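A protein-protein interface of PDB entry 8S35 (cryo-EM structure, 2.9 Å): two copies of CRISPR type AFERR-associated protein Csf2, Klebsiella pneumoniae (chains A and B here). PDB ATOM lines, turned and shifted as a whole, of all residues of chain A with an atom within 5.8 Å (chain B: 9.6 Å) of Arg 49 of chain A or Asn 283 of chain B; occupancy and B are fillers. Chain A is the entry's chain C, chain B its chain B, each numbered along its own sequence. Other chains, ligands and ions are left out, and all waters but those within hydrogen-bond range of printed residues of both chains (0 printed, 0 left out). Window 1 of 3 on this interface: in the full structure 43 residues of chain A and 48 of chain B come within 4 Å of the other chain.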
ATOM      1  N   PRO A  44       7.118  10.004   8.245  1.00  0.00           N
ATOM      2  CA  PRO A  44       5.927  10.796   8.568  1.00  0.00           C
ATOM      3  C   PRO A  44       5.700  10.898  10.066  1.00  0.00           C
ATOM      4  O   PRO A  44       5.895   9.937  10.812  1.00  0.00           O
ATOM      5  CB  PRO A  44       4.784  10.032   7.890  1.00  0.00           C
ATOM      6  CG  PRO A  44       5.414   9.121   6.936  1.00  0.00           C
ATOM      7  CD  PRO A  44       6.774   8.817   7.445  1.00  0.00           C
ATOM      8  N   GLY A  45       5.279  12.085  10.501  1.00  0.00           N
ATOM      9  CA  GLY A  45       4.777  12.221  11.852  1.00  0.00           C
ATOM     10  C   GLY A  45       3.478  11.482  12.070  1.00  0.00           C
ATOM     11  O   GLY A  45       3.108  11.222  13.217  1.00  0.00           O
ATOM     12  N   THR A  46       2.788  11.118  10.988  1.00  0.00           N
ATOM     13  CA  THR A  46       1.533  10.388  11.112  1.00  0.00           C
ATOM     14  C   THR A  46       1.773   8.979  11.632  1.00  0.00           C
ATOM     15  O   THR A  46       1.067   8.512  12.530  1.00  0.00           O
ATOM     16  CB  THR A  46       0.815  10.342   9.765  1.00  0.00           C
ATOM     17  OG1 THR A  46       1.577   9.553   8.843  1.00  0.00           O
ATOM     18  CG2 THR A  46       0.638  11.742   9.203  1.00  0.00           C
ATOM     19  N   SER A  47       2.752   8.275  11.062  1.00  0.00           N
ATOM     20  CA  SER A  47       3.033   6.918  11.519  1.00  0.00           C
ATOM     21  C   SER A  47       3.532   6.919  12.958  1.00  0.00           C
ATOM     22  O   SER A  47       3.129   6.071  13.762  1.00  0.00           O
ATOM     23  CB  SER A  47       4.055   6.258  10.597  1.00  0.00           C
ATOM     24  OG  SER A  47       3.496   6.015   9.318  1.00  0.00           O
ATOM     25  N   ILE A  48       4.396   7.874  13.305  1.00  0.00           N
ATOM     26  CA  ILE A  48       4.863   7.984  14.683  1.00  0.00           C
ATOM     27  C   ILE A  48       3.687   8.245  15.610  1.00  0.00           C
ATOM     28  O   ILE A  48       3.556   7.628  16.674  1.00  0.00           O
ATOM     29  CB  ILE A  48       5.924   9.091  14.818  1.00  0.00           C
ATOM     30  CG1 ILE A  48       7.106   8.869  13.865  1.00  0.00           C
ATOM     31  CG2 ILE A  48       6.403   9.161  16.254  1.00  0.00           C
ATOM     32  CD1 ILE A  48       7.903   7.608  14.123  1.00  0.00           C
ATOM     33  N   ARG A  49       2.825   9.184  15.225  1.00  0.00           N
ATOM     34  CA  ARG A  49       1.693   9.551  16.063  1.00  0.00           C
ATOM     35  C   ARG A  49       0.754   8.372  16.253  1.00  0.00           C
ATOM     36  O   ARG A  49       0.282   8.124  17.364  1.00  0.00           O
ATOM     37  CB  ARG A  49       0.960  10.734  15.435  1.00  0.00           C
ATOM     38  CG  ARG A  49      -0.243  11.235  16.214  1.00  0.00           C
ATOM     39  CD  ARG A  49      -0.747  12.553  15.636  1.00  0.00           C
ATOM     40  NE  ARG A  49      -1.041  13.573  16.638  1.00  0.00           N
ATOM     41  CZ  ARG A  49      -1.971  13.482  17.580  1.00  0.00           C
ATOM     42  NH1 ARG A  49      -2.667  12.374  17.769  1.00  0.00           N
ATOM     43  NH2 ARG A  49      -2.211  14.534  18.353  1.00  0.00           N
ATOM     44  N   GLY A  50       0.479   7.627  15.185  1.00  0.00           N
ATOM     45  CA  GLY A  50      -0.371   6.457  15.318  1.00  0.00           C
ATOM     46  C   GLY A  50       0.253   5.382  16.185  1.00  0.00           C
ATOM     47  O   GLY A  50      -0.429   4.752  16.996  1.00  0.00           O
ATOM     48  N   THR A  51       1.559   5.156  16.027  1.00  0.00           N
ATOM     49  CA  THR A  51       2.240   4.164  16.850  1.00  0.00           C
ATOM     50  C   THR A  51       2.154   4.532  18.324  1.00  0.00           C
ATOM     51  O   THR A  51       1.793   3.700  19.165  1.00  0.00           O
ATOM     52  CB  THR A  51       3.699   4.035  16.415  1.00  0.00           C
ATOM     53  OG1 THR A  51       3.757   3.550  15.069  1.00  0.00           O
ATOM     54  CG2 THR A  51       4.444   3.075  17.328  1.00  0.00           C
ATOM     55  N   LEU A  52       2.472   5.782  18.656  1.00  0.00           N
ATOM     56  CA  LEU A  52       2.414   6.190  20.053  1.00  0.00           C
ATOM     57  C   LEU A  52       0.981   6.236  20.559  1.00  0.00           C
ATOM     58  O   LEU A  52       0.743   5.986  21.742  1.00  0.00           O
ATOM     59  CB  LEU A  52       3.084   7.551  20.256  1.00  0.00           C
ATOM     60  CG  LEU A  52       4.610   7.640  20.392  1.00  0.00           C
ATOM     61  CD1 LEU A  52       5.205   6.580  21.316  1.00  0.00           C
ATOM     62  CD2 LEU A  52       5.268   7.572  19.037  1.00  0.00           C
ATOM     63  N   ARG A  53       0.017   6.541  19.693  1.00  0.00           N
ATOM     64  CA  ARG A  53      -1.373   6.529  20.123  1.00  0.00           C
ATOM     65  C   ARG A  53      -1.823   5.116  20.456  1.00  0.00           C
ATOM     66  O   ARG A  53      -2.525   4.902  21.448  1.00  0.00           O
ATOM     67  CB  ARG A  53      -2.265   7.136  19.044  1.00  0.00           C
ATOM     68  CG  ARG A  53      -3.701   7.313  19.488  1.00  0.00           C
ATOM     69  CD  ARG A  53      -4.450   8.300  18.615  1.00  0.00           C
ATOM     70  NE  ARG A  53      -5.782   8.572  19.145  1.00  0.00           N
ATOM     71  CZ  ARG A  53      -6.530   9.618  18.820  1.00  0.00           C
ATOM     72  NH1 ARG A  53      -6.111  10.533  17.960  1.00  0.00           N
ATOM     73  NH2 ARG A  53      -7.729   9.754  19.377  1.00  0.00           N
ATOM     74  N   HIS A  54      -1.421   4.136  19.648  1.00  0.00           N
ATOM     75  CA  HIS A  54      -1.752   2.752  19.965  1.00  0.00           C
ATOM     76  C   HIS A  54      -1.033   2.299  21.227  1.00  0.00           C
ATOM     77  O   HIS A  54      -1.594   1.550  22.036  1.00  0.00           O
ATOM     78  CB  HIS A  54      -1.404   1.845  18.789  1.00  0.00           C
ATOM     79  CG  HIS A  54      -2.475   1.777  17.749  1.00  0.00           C
ATOM     80  ND1 HIS A  54      -2.947   2.895  17.096  1.00  0.00           N
ATOM     81  CD2 HIS A  54      -3.172   0.728  17.253  1.00  0.00           C
ATOM     82  CE1 HIS A  54      -3.886   2.536  16.238  1.00  0.00           C
ATOM     83  NE2 HIS A  54      -4.043   1.227  16.315  1.00  0.00           N
ATOM     84  N   LEU A 115      -4.860  14.010  25.239  1.00  0.00           N
ATOM     85  CA  LEU A 115      -3.540  13.952  24.631  1.00  0.00           C
ATOM     86  C   LEU A 115      -3.648  13.803  23.121  1.00  0.00           C
ATOM     87  O   LEU A 115      -3.255  14.697  22.365  1.00  0.00           O
ATOM     88  CB  LEU A 115      -2.768  12.786  25.251  1.00  0.00           C
ATOM     89  CG  LEU A 115      -1.253  12.702  25.098  1.00  0.00           C
ATOM     90  CD1 LEU A 115      -0.580  13.900  25.733  1.00  0.00           C
ATOM     91  CD2 LEU A 115      -0.747  11.417  25.733  1.00  0.00           C
ATOM     92  N   PHE A 116      -4.245  12.703  22.667  1.00  0.00           N
ATOM     93  CA  PHE A 116      -4.528  12.466  21.257  1.00  0.00           C
ATOM     94  C   PHE A 116      -5.980  12.855  21.013  1.00  0.00           C
ATOM     95  O   PHE A 116      -6.895  12.166  21.475  1.00  0.00           O
ATOM     96  CB  PHE A 116      -4.274  11.009  20.881  1.00  0.00           C
ATOM     97  CG  PHE A 116      -2.908  10.510  21.265  1.00  0.00           C
ATOM     98  CD1 PHE A 116      -2.661  10.034  22.540  1.00  0.00           C
ATOM     99  CD2 PHE A 116      -1.875  10.509  20.348  1.00  0.00           C
ATOM    100  CE1 PHE A 116      -1.410   9.575  22.891  1.00  0.00           C
ATOM    101  CE2 PHE A 116      -0.623  10.050  20.694  1.00  0.00           C
ATOM    102  CZ  PHE A 116      -0.391   9.583  21.966  1.00  0.00           C
ATOM    103  N   GLY A 117      -6.194  13.932  20.272  1.00  0.00           N
ATOM    104  CA  GLY A 117      -7.530  14.457  20.111  1.00  0.00           C
ATOM    105  C   GLY A 117      -8.430  13.517  19.328  1.00  0.00           C
ATOM    106  O   GLY A 117      -8.099  12.371  19.023  1.00  0.00           O
ATOM    107  N   GLY A 123      -6.149  17.867  19.689  1.00  0.00           N
ATOM    108  CA  GLY A 123      -5.218  16.964  20.333  1.00  0.00           C
ATOM    109  C   GLY A 123      -4.069  17.709  20.976  1.00  0.00           C
ATOM    110  O   GLY A 123      -3.293  18.375  20.284  1.00  0.00           O
ATOM    111  N   LYS A 124      -3.953  17.613  22.301  1.00  0.00           N
ATOM    112  CA  LYS A 124      -2.890  18.330  22.997  1.00  0.00           C
ATOM    113  C   LYS A 124      -1.511  17.884  22.535  1.00  0.00           C
ATOM    114  O   LYS A 124      -0.572  18.687  22.529  1.00  0.00           O
ATOM    115  CB  LYS A 124      -3.026  18.137  24.506  1.00  0.00           C
ATOM    116  CG  LYS A 124      -3.918  19.162  25.176  1.00  0.00           C
ATOM    117  CD  LYS A 124      -3.946  18.972  26.680  1.00  0.00           C
ATOM    118  CE  LYS A 124      -4.682  20.105  27.368  1.00  0.00           C
ATOM    119  NZ  LYS A 124      -4.734  19.919  28.844  1.00  0.00           N
ATOM    120  N   VAL A 125      -1.366  16.624  22.137  1.00  0.00           N
ATOM    121  CA  VAL A 125      -0.083  16.092  21.698  1.00  0.00           C
ATOM    122  C   VAL A 125       0.044  16.279  20.194  1.00  0.00           C
ATOM    123  O   VAL A 125      -0.878  15.961  19.435  1.00  0.00           O
ATOM    124  CB  VAL A 125       0.073  14.612  22.097  1.00  0.00           C
ATOM    125  CG1 VAL A 125      -0.699  13.680  21.170  1.00  0.00           C
ATOM    126  CG2 VAL A 125       1.541  14.228  22.121  1.00  0.00           C
ATOM    127  N   GLY A 126       1.162  16.854  19.770  1.00  0.00           N
ATOM    128  CA  GLY A 126       1.484  17.002  18.369  1.00  0.00           C
ATOM    129  C   GLY A 126       2.836  16.386  18.099  1.00  0.00           C
ATOM    130  O   GLY A 126       3.843  16.845  18.645  1.00  0.00           O
ATOM    131  N   ILE A 127       2.880  15.351  17.267  1.00  0.00           N
ATOM    132  CA  ILE A 127       4.107  14.616  16.991  1.00  0.00           C
ATOM    133  C   ILE A 127       4.619  15.057  15.631  1.00  0.00           C
ATOM    134  O   ILE A 127       3.947  14.865  14.612  1.00  0.00           O
ATOM    135  CB  ILE A 127       3.884  13.093  17.023  1.00  0.00           C
ATOM    136  CG1 ILE A 127       3.236  12.630  18.341  1.00  0.00           C
ATOM    137  CG2 ILE A 127       5.217  12.371  16.822  1.00  0.00           C
ATOM    138  CD1 ILE A 127       1.766  12.913  18.469  1.00  0.00           C
ATOM    139  N   GLY A 128       5.819  15.629  15.609  1.00  0.00           N
ATOM    140  CA  GLY A 128       6.388  16.118  14.378  1.00  0.00           C
ATOM    141  C   GLY A 128       6.980  15.013  13.536  1.00  0.00           C
ATOM    142  O   GLY A 128       7.020  13.841  13.908  1.00  0.00           O
ATOM    143  N   GLU B  14       8.966  22.341  12.117  1.00  0.00           N
ATOM    144  CA  GLU B  14       8.083  21.279  11.672  1.00  0.00           C
ATOM    145  C   GLU B  14       7.181  21.869  10.600  1.00  0.00           C
ATOM    146  O   GLU B  14       6.935  23.078  10.613  1.00  0.00           O
ATOM    147  CB  GLU B  14       7.243  20.724  12.832  1.00  0.00           C
ATOM    148  CG  GLU B  14       7.312  19.210  13.024  1.00  0.00           C
ATOM    149  CD  GLU B  14       8.722  18.696  13.232  1.00  0.00           C
ATOM    150  OE1 GLU B  14       8.960  17.496  12.977  1.00  0.00           O
ATOM    151  OE2 GLU B  14       9.589  19.487  13.657  1.00  0.00           O
ATOM    152  N   PRO B  15       6.675  21.054   9.669  1.00  0.00           N
ATOM    153  CA  PRO B  15       6.036  21.608   8.466  1.00  0.00           C
ATOM    154  C   PRO B  15       4.945  22.621   8.779  1.00  0.00           C
ATOM    155  O   PRO B  15       4.134  22.434   9.686  1.00  0.00           O
ATOM    156  CB  PRO B  15       5.460  20.371   7.769  1.00  0.00           C
ATOM    157  CG  PRO B  15       6.247  19.246   8.274  1.00  0.00           C
ATOM    158  CD  PRO B  15       6.615  19.584   9.679  1.00  0.00           C
ATOM    159  N   THR B  17       1.658  24.639   7.725  1.00  0.00           N
ATOM    160  CA  THR B  17       0.482  24.419   6.895  1.00  0.00           C
ATOM    161  C   THR B  17      -0.634  25.360   7.317  1.00  0.00           C
ATOM    162  O   THR B  17      -0.674  25.847   8.448  1.00  0.00           O
ATOM    163  CB  THR B  17      -0.013  22.973   6.990  1.00  0.00           C
ATOM    164  OG1 THR B  17      -0.973  22.726   5.957  1.00  0.00           O
ATOM    165  CG2 THR B  17      -0.654  22.713   8.342  1.00  0.00           C
ATOM    166  N   PHE B 141       2.543  17.117   2.688  1.00  0.00           N
ATOM    167  CA  PHE B 141       2.792  16.448   3.952  1.00  0.00           C
ATOM    168  C   PHE B 141       1.510  15.781   4.442  1.00  0.00           C
ATOM    169  O   PHE B 141       0.463  15.816   3.787  1.00  0.00           O
ATOM    170  CB  PHE B 141       3.338  17.445   4.968  1.00  0.00           C
ATOM    171  CG  PHE B 141       4.761  17.821   4.725  1.00  0.00           C
ATOM    172  CD1 PHE B 141       5.085  18.781   3.787  1.00  0.00           C
ATOM    173  CD2 PHE B 141       5.779  17.206   5.426  1.00  0.00           C
ATOM    174  CE1 PHE B 141       6.398  19.125   3.559  1.00  0.00           C
ATOM    175  CE2 PHE B 141       7.092  17.546   5.202  1.00  0.00           C
ATOM    176  CZ  PHE B 141       7.402  18.505   4.267  1.00  0.00           C
ATOM    177  N   GLY B 142       1.584  15.182   5.624  1.00  0.00           N
ATOM    178  CA  GLY B 142       0.438  14.451   6.130  1.00  0.00           C
ATOM    179  C   GLY B 142       0.252  13.184   5.329  1.00  0.00           C
ATOM    180  O   GLY B 142       1.196  12.417   5.110  1.00  0.00           O
ATOM    181  N   GLY B 143      -0.971  12.955   4.884  1.00  0.00           N
ATOM    182  CA  GLY B 143      -1.226  11.775   4.102  1.00  0.00           C
ATOM    183  C   GLY B 143      -1.208  10.529   4.970  1.00  0.00           C
ATOM    184  O   GLY B 143      -1.236  10.574   6.199  1.00  0.00           O
ATOM    185  N   ILE B 236      -5.861   9.090   4.099  1.00  0.00           N
ATOM    186  CA  ILE B 236      -5.945  10.483   4.514  1.00  0.00           C
ATOM    187  C   ILE B 236      -5.413  11.352   3.385  1.00  0.00           C
ATOM    188  O   ILE B 236      -4.304  11.132   2.885  1.00  0.00           O
ATOM    189  CB  ILE B 236      -5.151  10.719   5.809  1.00  0.00           C
ATOM    190  CG1 ILE B 236      -5.492   9.661   6.863  1.00  0.00           C
ATOM    191  CG2 ILE B 236      -5.408  12.120   6.352  1.00  0.00           C
ATOM    192  CD1 ILE B 236      -6.975   9.398   7.045  1.00  0.00           C
ATOM    193  N   ASP B 237      -6.203  12.329   2.973  1.00  0.00           N
ATOM    194  CA  ASP B 237      -5.763  13.225   1.920  1.00  0.00           C
ATOM    195  C   ASP B 237      -4.596  14.060   2.440  1.00  0.00           C
ATOM    196  O   ASP B 237      -4.723  14.689   3.497  1.00  0.00           O
ATOM    197  CB  ASP B 237      -6.907  14.132   1.477  1.00  0.00           C
ATOM    198  CG  ASP B 237      -8.157  13.356   1.117  1.00  0.00           C
ATOM    199  OD1 ASP B 237      -8.028  12.250   0.553  1.00  0.00           O
ATOM    200  OD2 ASP B 237      -9.267  13.851   1.402  1.00  0.00           O
ATOM    201  N   TYR B 239      -2.008  17.180   3.000  1.00  0.00           N
ATOM    202  CA  TYR B 239      -2.152  18.628   3.017  1.00  0.00           C
ATOM    203  C   TYR B 239      -0.858  19.268   2.540  1.00  0.00           C
ATOM    204  O   TYR B 239       0.234  18.816   2.890  1.00  0.00           O
ATOM    205  CB  TYR B 239      -2.515  19.141   4.414  1.00  0.00           C
ATOM    206  CG  TYR B 239      -1.562  18.731   5.513  1.00  0.00           C
ATOM    207  CD1 TYR B 239      -0.378  19.418   5.726  1.00  0.00           C
ATOM    208  CD2 TYR B 239      -1.858  17.668   6.351  1.00  0.00           C
ATOM    209  CE1 TYR B 239       0.488  19.051   6.725  1.00  0.00           C
ATOM    210  CE2 TYR B 239      -0.998  17.298   7.362  1.00  0.00           C
ATOM    211  CZ  TYR B 239       0.176  17.990   7.542  1.00  0.00           C
ATOM    212  OH  TYR B 239       1.042  17.624   8.545  1.00  0.00           O
ATOM    213  N   GLU B 275       4.847  28.878  22.607  1.00  0.00           N
ATOM    214  CA  GLU B 275       4.149  27.943  21.724  1.00  0.00           C
ATOM    215  C   GLU B 275       4.254  28.490  20.307  1.00  0.00           C
ATOM    216  O   GLU B 275       3.278  29.004  19.749  1.00  0.00           O
ATOM    217  CB  GLU B 275       2.691  27.762  22.149  1.00  0.00           C
ATOM    218  CG  GLU B 275       1.878  26.806  21.275  1.00  0.00           C
ATOM    219  CD  GLU B 275       2.504  25.430  21.159  1.00  0.00           C
ATOM    220  OE1 GLU B 275       3.200  25.010  22.106  1.00  0.00           O
ATOM    221  OE2 GLU B 275       2.303  24.770  20.118  1.00  0.00           O
ATOM    222  N   ARG B 277       3.633  28.207  17.324  1.00  0.00           N
ATOM    223  CA  ARG B 277       2.860  27.437  16.361  1.00  0.00           C
ATOM    224  C   ARG B 277       2.097  28.379  15.443  1.00  0.00           C
ATOM    225  O   ARG B 277       1.398  29.283  15.913  1.00  0.00           O
ATOM    226  CB  ARG B 277       1.886  26.496  17.072  1.00  0.00           C
ATOM    227  CG  ARG B 277       1.529  25.257  16.264  1.00  0.00           C
ATOM    228  CD  ARG B 277       0.959  24.155  17.139  1.00  0.00           C
ATOM    229  NE  ARG B 277       1.942  23.641  18.085  1.00  0.00           N
ATOM    230  CZ  ARG B 277       2.991  22.899  17.754  1.00  0.00           C
ATOM    231  NH1 ARG B 277       3.220  22.537  16.502  1.00  0.00           N
ATOM    232  NH2 ARG B 277       3.832  22.508  18.706  1.00  0.00           N
ATOM    233  N   GLY B 279      -0.461  27.881  12.405  1.00  0.00           N
ATOM    234  CA  GLY B 279      -1.325  27.192  11.467  1.00  0.00           C
ATOM    235  C   GLY B 279      -1.948  25.947  12.071  1.00  0.00           C
ATOM    236  O   GLY B 279      -2.127  25.850  13.292  1.00  0.00           O
ATOM    237  N   GLY B 280      -2.268  24.992  11.195  1.00  0.00           N
ATOM    238  CA  GLY B 280      -3.044  23.833  11.547  1.00  0.00           C
ATOM    239  C   GLY B 280      -2.254  22.542  11.526  1.00  0.00           C
ATOM    240  O   GLY B 280      -1.016  22.530  11.544  1.00  0.00           O
ATOM    241  N   HIS B 281      -2.992  21.436  11.451  1.00  0.00           N
ATOM    242  CA  HIS B 281      -2.477  20.080  11.624  1.00  0.00           C
ATOM    243  C   HIS B 281      -1.469  20.011  12.766  1.00  0.00           C
ATOM    244  O   HIS B 281      -0.384  19.438  12.650  1.00  0.00           O
ATOM    245  CB  HIS B 281      -1.884  19.563  10.321  1.00  0.00           C
ATOM    246  CG  HIS B 281      -2.884  19.470   9.213  1.00  0.00           C
ATOM    247  ND1 HIS B 281      -3.014  20.441   8.244  1.00  0.00           N
ATOM    248  CD2 HIS B 281      -3.818  18.531   8.932  1.00  0.00           C
ATOM    249  CE1 HIS B 281      -3.978  20.098   7.408  1.00  0.00           C
ATOM    250  NE2 HIS B 281      -4.481  18.944   7.802  1.00  0.00           N
ATOM    251  N   ALA B 282      -1.859  20.587  13.904  1.00  0.00           N
ATOM    252  CA  ALA B 282      -1.039  20.500  15.103  1.00  0.00           C
ATOM    253  C   ALA B 282      -0.923  19.071  15.613  1.00  0.00           C
ATOM    254  O   ALA B 282      -0.027  18.786  16.411  1.00  0.00           O
ATOM    255  CB  ALA B 282      -1.612  21.395  16.200  1.00  0.00           C
ATOM    256  N   ASN B 283      -1.809  18.174  15.174  1.00  0.00           N
ATOM    257  CA  ASN B 283      -1.681  16.771  15.550  1.00  0.00           C
ATOM    258  C   ASN B 283      -0.344  16.213  15.090  1.00  0.00           C
ATOM    259  O   ASN B 283       0.253  15.367  15.765  1.00  0.00           O
ATOM    260  CB  ASN B 283      -2.834  15.962  14.958  1.00  0.00           C
ATOM    261  CG  ASN B 283      -2.893  16.049  13.448  1.00  0.00           C
ATOM    262  OD1 ASN B 283      -2.125  16.784  12.827  1.00  0.00           O
ATOM    263  ND2 ASN B 283      -3.804  15.294  12.847  1.00  0.00           N
ATOM    264  N   HIS B 284       0.140  16.671  13.936  1.00  0.00           N
ATOM    265  CA  HIS B 284       1.461  16.319  13.441  1.00  0.00           C
ATOM    266  C   HIS B 284       2.505  17.363  13.818  1.00  0.00           C
ATOM    267  O   HIS B 284       3.535  17.474  13.148  1.00  0.00           O
ATOM    268  CB  HIS B 284       1.414  16.129  11.927  1.00  0.00           C
ATOM    269  CG  HIS B 284       0.248  15.313  11.466  1.00  0.00           C
ATOM    270  ND1 HIS B 284      -0.454  15.600  10.316  1.00  0.00           N
ATOM    271  CD2 HIS B 284      -0.347  14.223  12.006  1.00  0.00           C
ATOM    272  CE1 HIS B 284      -1.427  14.720  10.164  1.00  0.00           C
ATOM    273  NE2 HIS B 284      -1.384  13.874  11.177  1.00  0.00           N
ATOM    274  N   ASN B 285       2.245  18.144  14.867  1.00  0.00           N
ATOM    275  CA  ASN B 285       3.158  19.167  15.367  1.00  0.00           C
ATOM    276  C   ASN B 285       3.454  20.243  14.331  1.00  0.00           C
ATOM    277  O   ASN B 285       4.447  20.966  14.454  1.00  0.00           O
ATOM    278  CB  ASN B 285       4.471  18.554  15.856  1.00  0.00           C
ATOM    279  CG  ASN B 285       5.177  19.424  16.874  1.00  0.00           C
ATOM    280  OD1 ASN B 285       4.745  20.542  17.157  1.00  0.00           O
ATOM    281  ND2 ASN B 285       6.267  18.916  17.434  1.00  0.00           N
ATOM    282  N   CYS B 286       2.619  20.372  13.308  1.00  0.00           N
ATOM    283  CA  CYS B 286       2.832  21.413  12.318  1.00  0.00           C
ATOM    284  C   CYS B 286       2.624  22.781  12.949  1.00  0.00           C
ATOM    285  O   CYS B 286       1.807  22.955  13.857  1.00  0.00           O
ATOM    286  CB  CYS B 286       1.886  21.232  11.136  1.00  0.00           C
ATOM    287  SG  CYS B 286       2.362  19.899  10.027  1.00  0.00           S
ATOM    288  N   GLY B 287       3.384  23.757  12.463  1.00  0.00           N
ATOM    289  CA  GLY B 287       3.325  25.115  12.951  1.00  0.00           C
ATOM    290  C   GLY B 287       4.555  25.560  13.706  1.00  0.00           C
ATOM    291  O   GLY B 287       4.803  26.770  13.791  1.00  0.00           O
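The backbone carbonyl oxygen (O) of Asn 283 of chain B is in hydrogen-bond range of the backbone NH (N) of Ile 127 of chain A, 3.0 Å away. The backbone carbonyl oxygen (O) of Gly 126 of chain A sits close to the side-chain amide nitrogen (ND2) of Asn 285 of chain B (3.4 Å). NE of Arg 49 of chain A lies close to O of Asn 283 of chain B (2.4 Å). The backbone carbonyl oxygen (O) of Ile 127 of chain A lies close to the backbone carbonyl oxygen (O) of His 284 of chain B.
The side-chain hydroxyl (OH) of Tyr 239 of chain B is in hydrogen-bond range of a ring nitrogen (ND1) of His 284 of chain B (3.1 Å). The guanidinium group (NH1) of Arg 277 of chain B lies within hydrogen-bond range of the side-chain amide oxygen (OD1) of Asn 285 of chain B (2.6 Å). The side-chain amide oxygen of Asn 283 of chain B lies close to the backbone carbonyl oxygen of His 281 of chain B (3.2 Å). OD1 of Asn 283 of chain B sits close to ND1 of His 284 of chain B, 3.2 Å away. The backbone carbonyl oxygen (O) of Leu 115 of chain A sits at hydrogen-bond distance from the backbone NH (N) of Val 125 of chain A (2.7 Å).
Among the printed residues, pairs that only touch across the chains: Thr 46 of chain A with Gly 143 of chain B (3.7 Å), Thr 46 of chain A with His 284 of chain B (3.5 Å), Val 125 of chain A with Asn 283 of chain B (3.9 Å), Gly 126 of chain A with Ala 282 of chain B (3.0 Å), Gly 126 of chain A with Asn 283 of chain B (3.3 Å), Ile 127 of chain A with Asn 285 of chain B (3.5 Å), Gly 128 of chain A with Glu 14 of chain B (3.2 Å), Gly 128 of chain A with His 284 of chain B (3.4 Å) and Gly 128 of chain A with Asn 285 of chain B (3.2 Å).
Of the printed residues of chain B, Arg 49 of chain A touches Asn 283. Of chain A, only Arg 49 (2.4 Å), Val 125 (3.9 Å), Gly 126 (3.3 Å) and Ile 127 (3.0 Å) come within 4 Å of Asn 283 of chain B. Val 125 of chain A touches just one residue of chain B: Asn 283. Of the printed residues of chain B, Gly 126 of chain A touches Ala 282 (3.0 Å), Asn 283 (3.3 Å) and Asn 285 (3.3 Å). Ile 127 of chain A touches just these residues of chain B: Asn 283 (3.0 Å), His 284 (3.0 Å) and Asn 285 (3.5 Å). Of the printed residues of chain A, Ala 282 of chain B touches Gly 126. Of the printed residues of chain A, His 284 of chain B touches Thr 46, Ile 127 and Gly 128. Of the printed residues of chain A, Gly 143 of chain B touches Thr 46. Of the printed residues of chain A, Asn 285 of chain B touches Gly 126, Ile 127 and Gly 128. Of the printed residues of chain B, Thr 46 of chain A touches Gly 143 (3.7 Å) and His 284 (3.5 Å). The nearest printed residue of chain B that does not touch Arg 49 of chain A is His 284 of chain B (4.02 Å).
Along chain A the printed residues that touch a printed residue of chain B span positions 46 to 128. Printed residues of chain B that touch a printed residue of chain A: Glu 14, Gly 143, Ala 282, Asn 283, His 284 and Asn 285. Among the printed residues, 13 pairs touch across the chains.
No position is printed for both chains. Of the 13 pairs that touch across the chains among the printed residues, none has its exchanged pair printed and touching as well.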
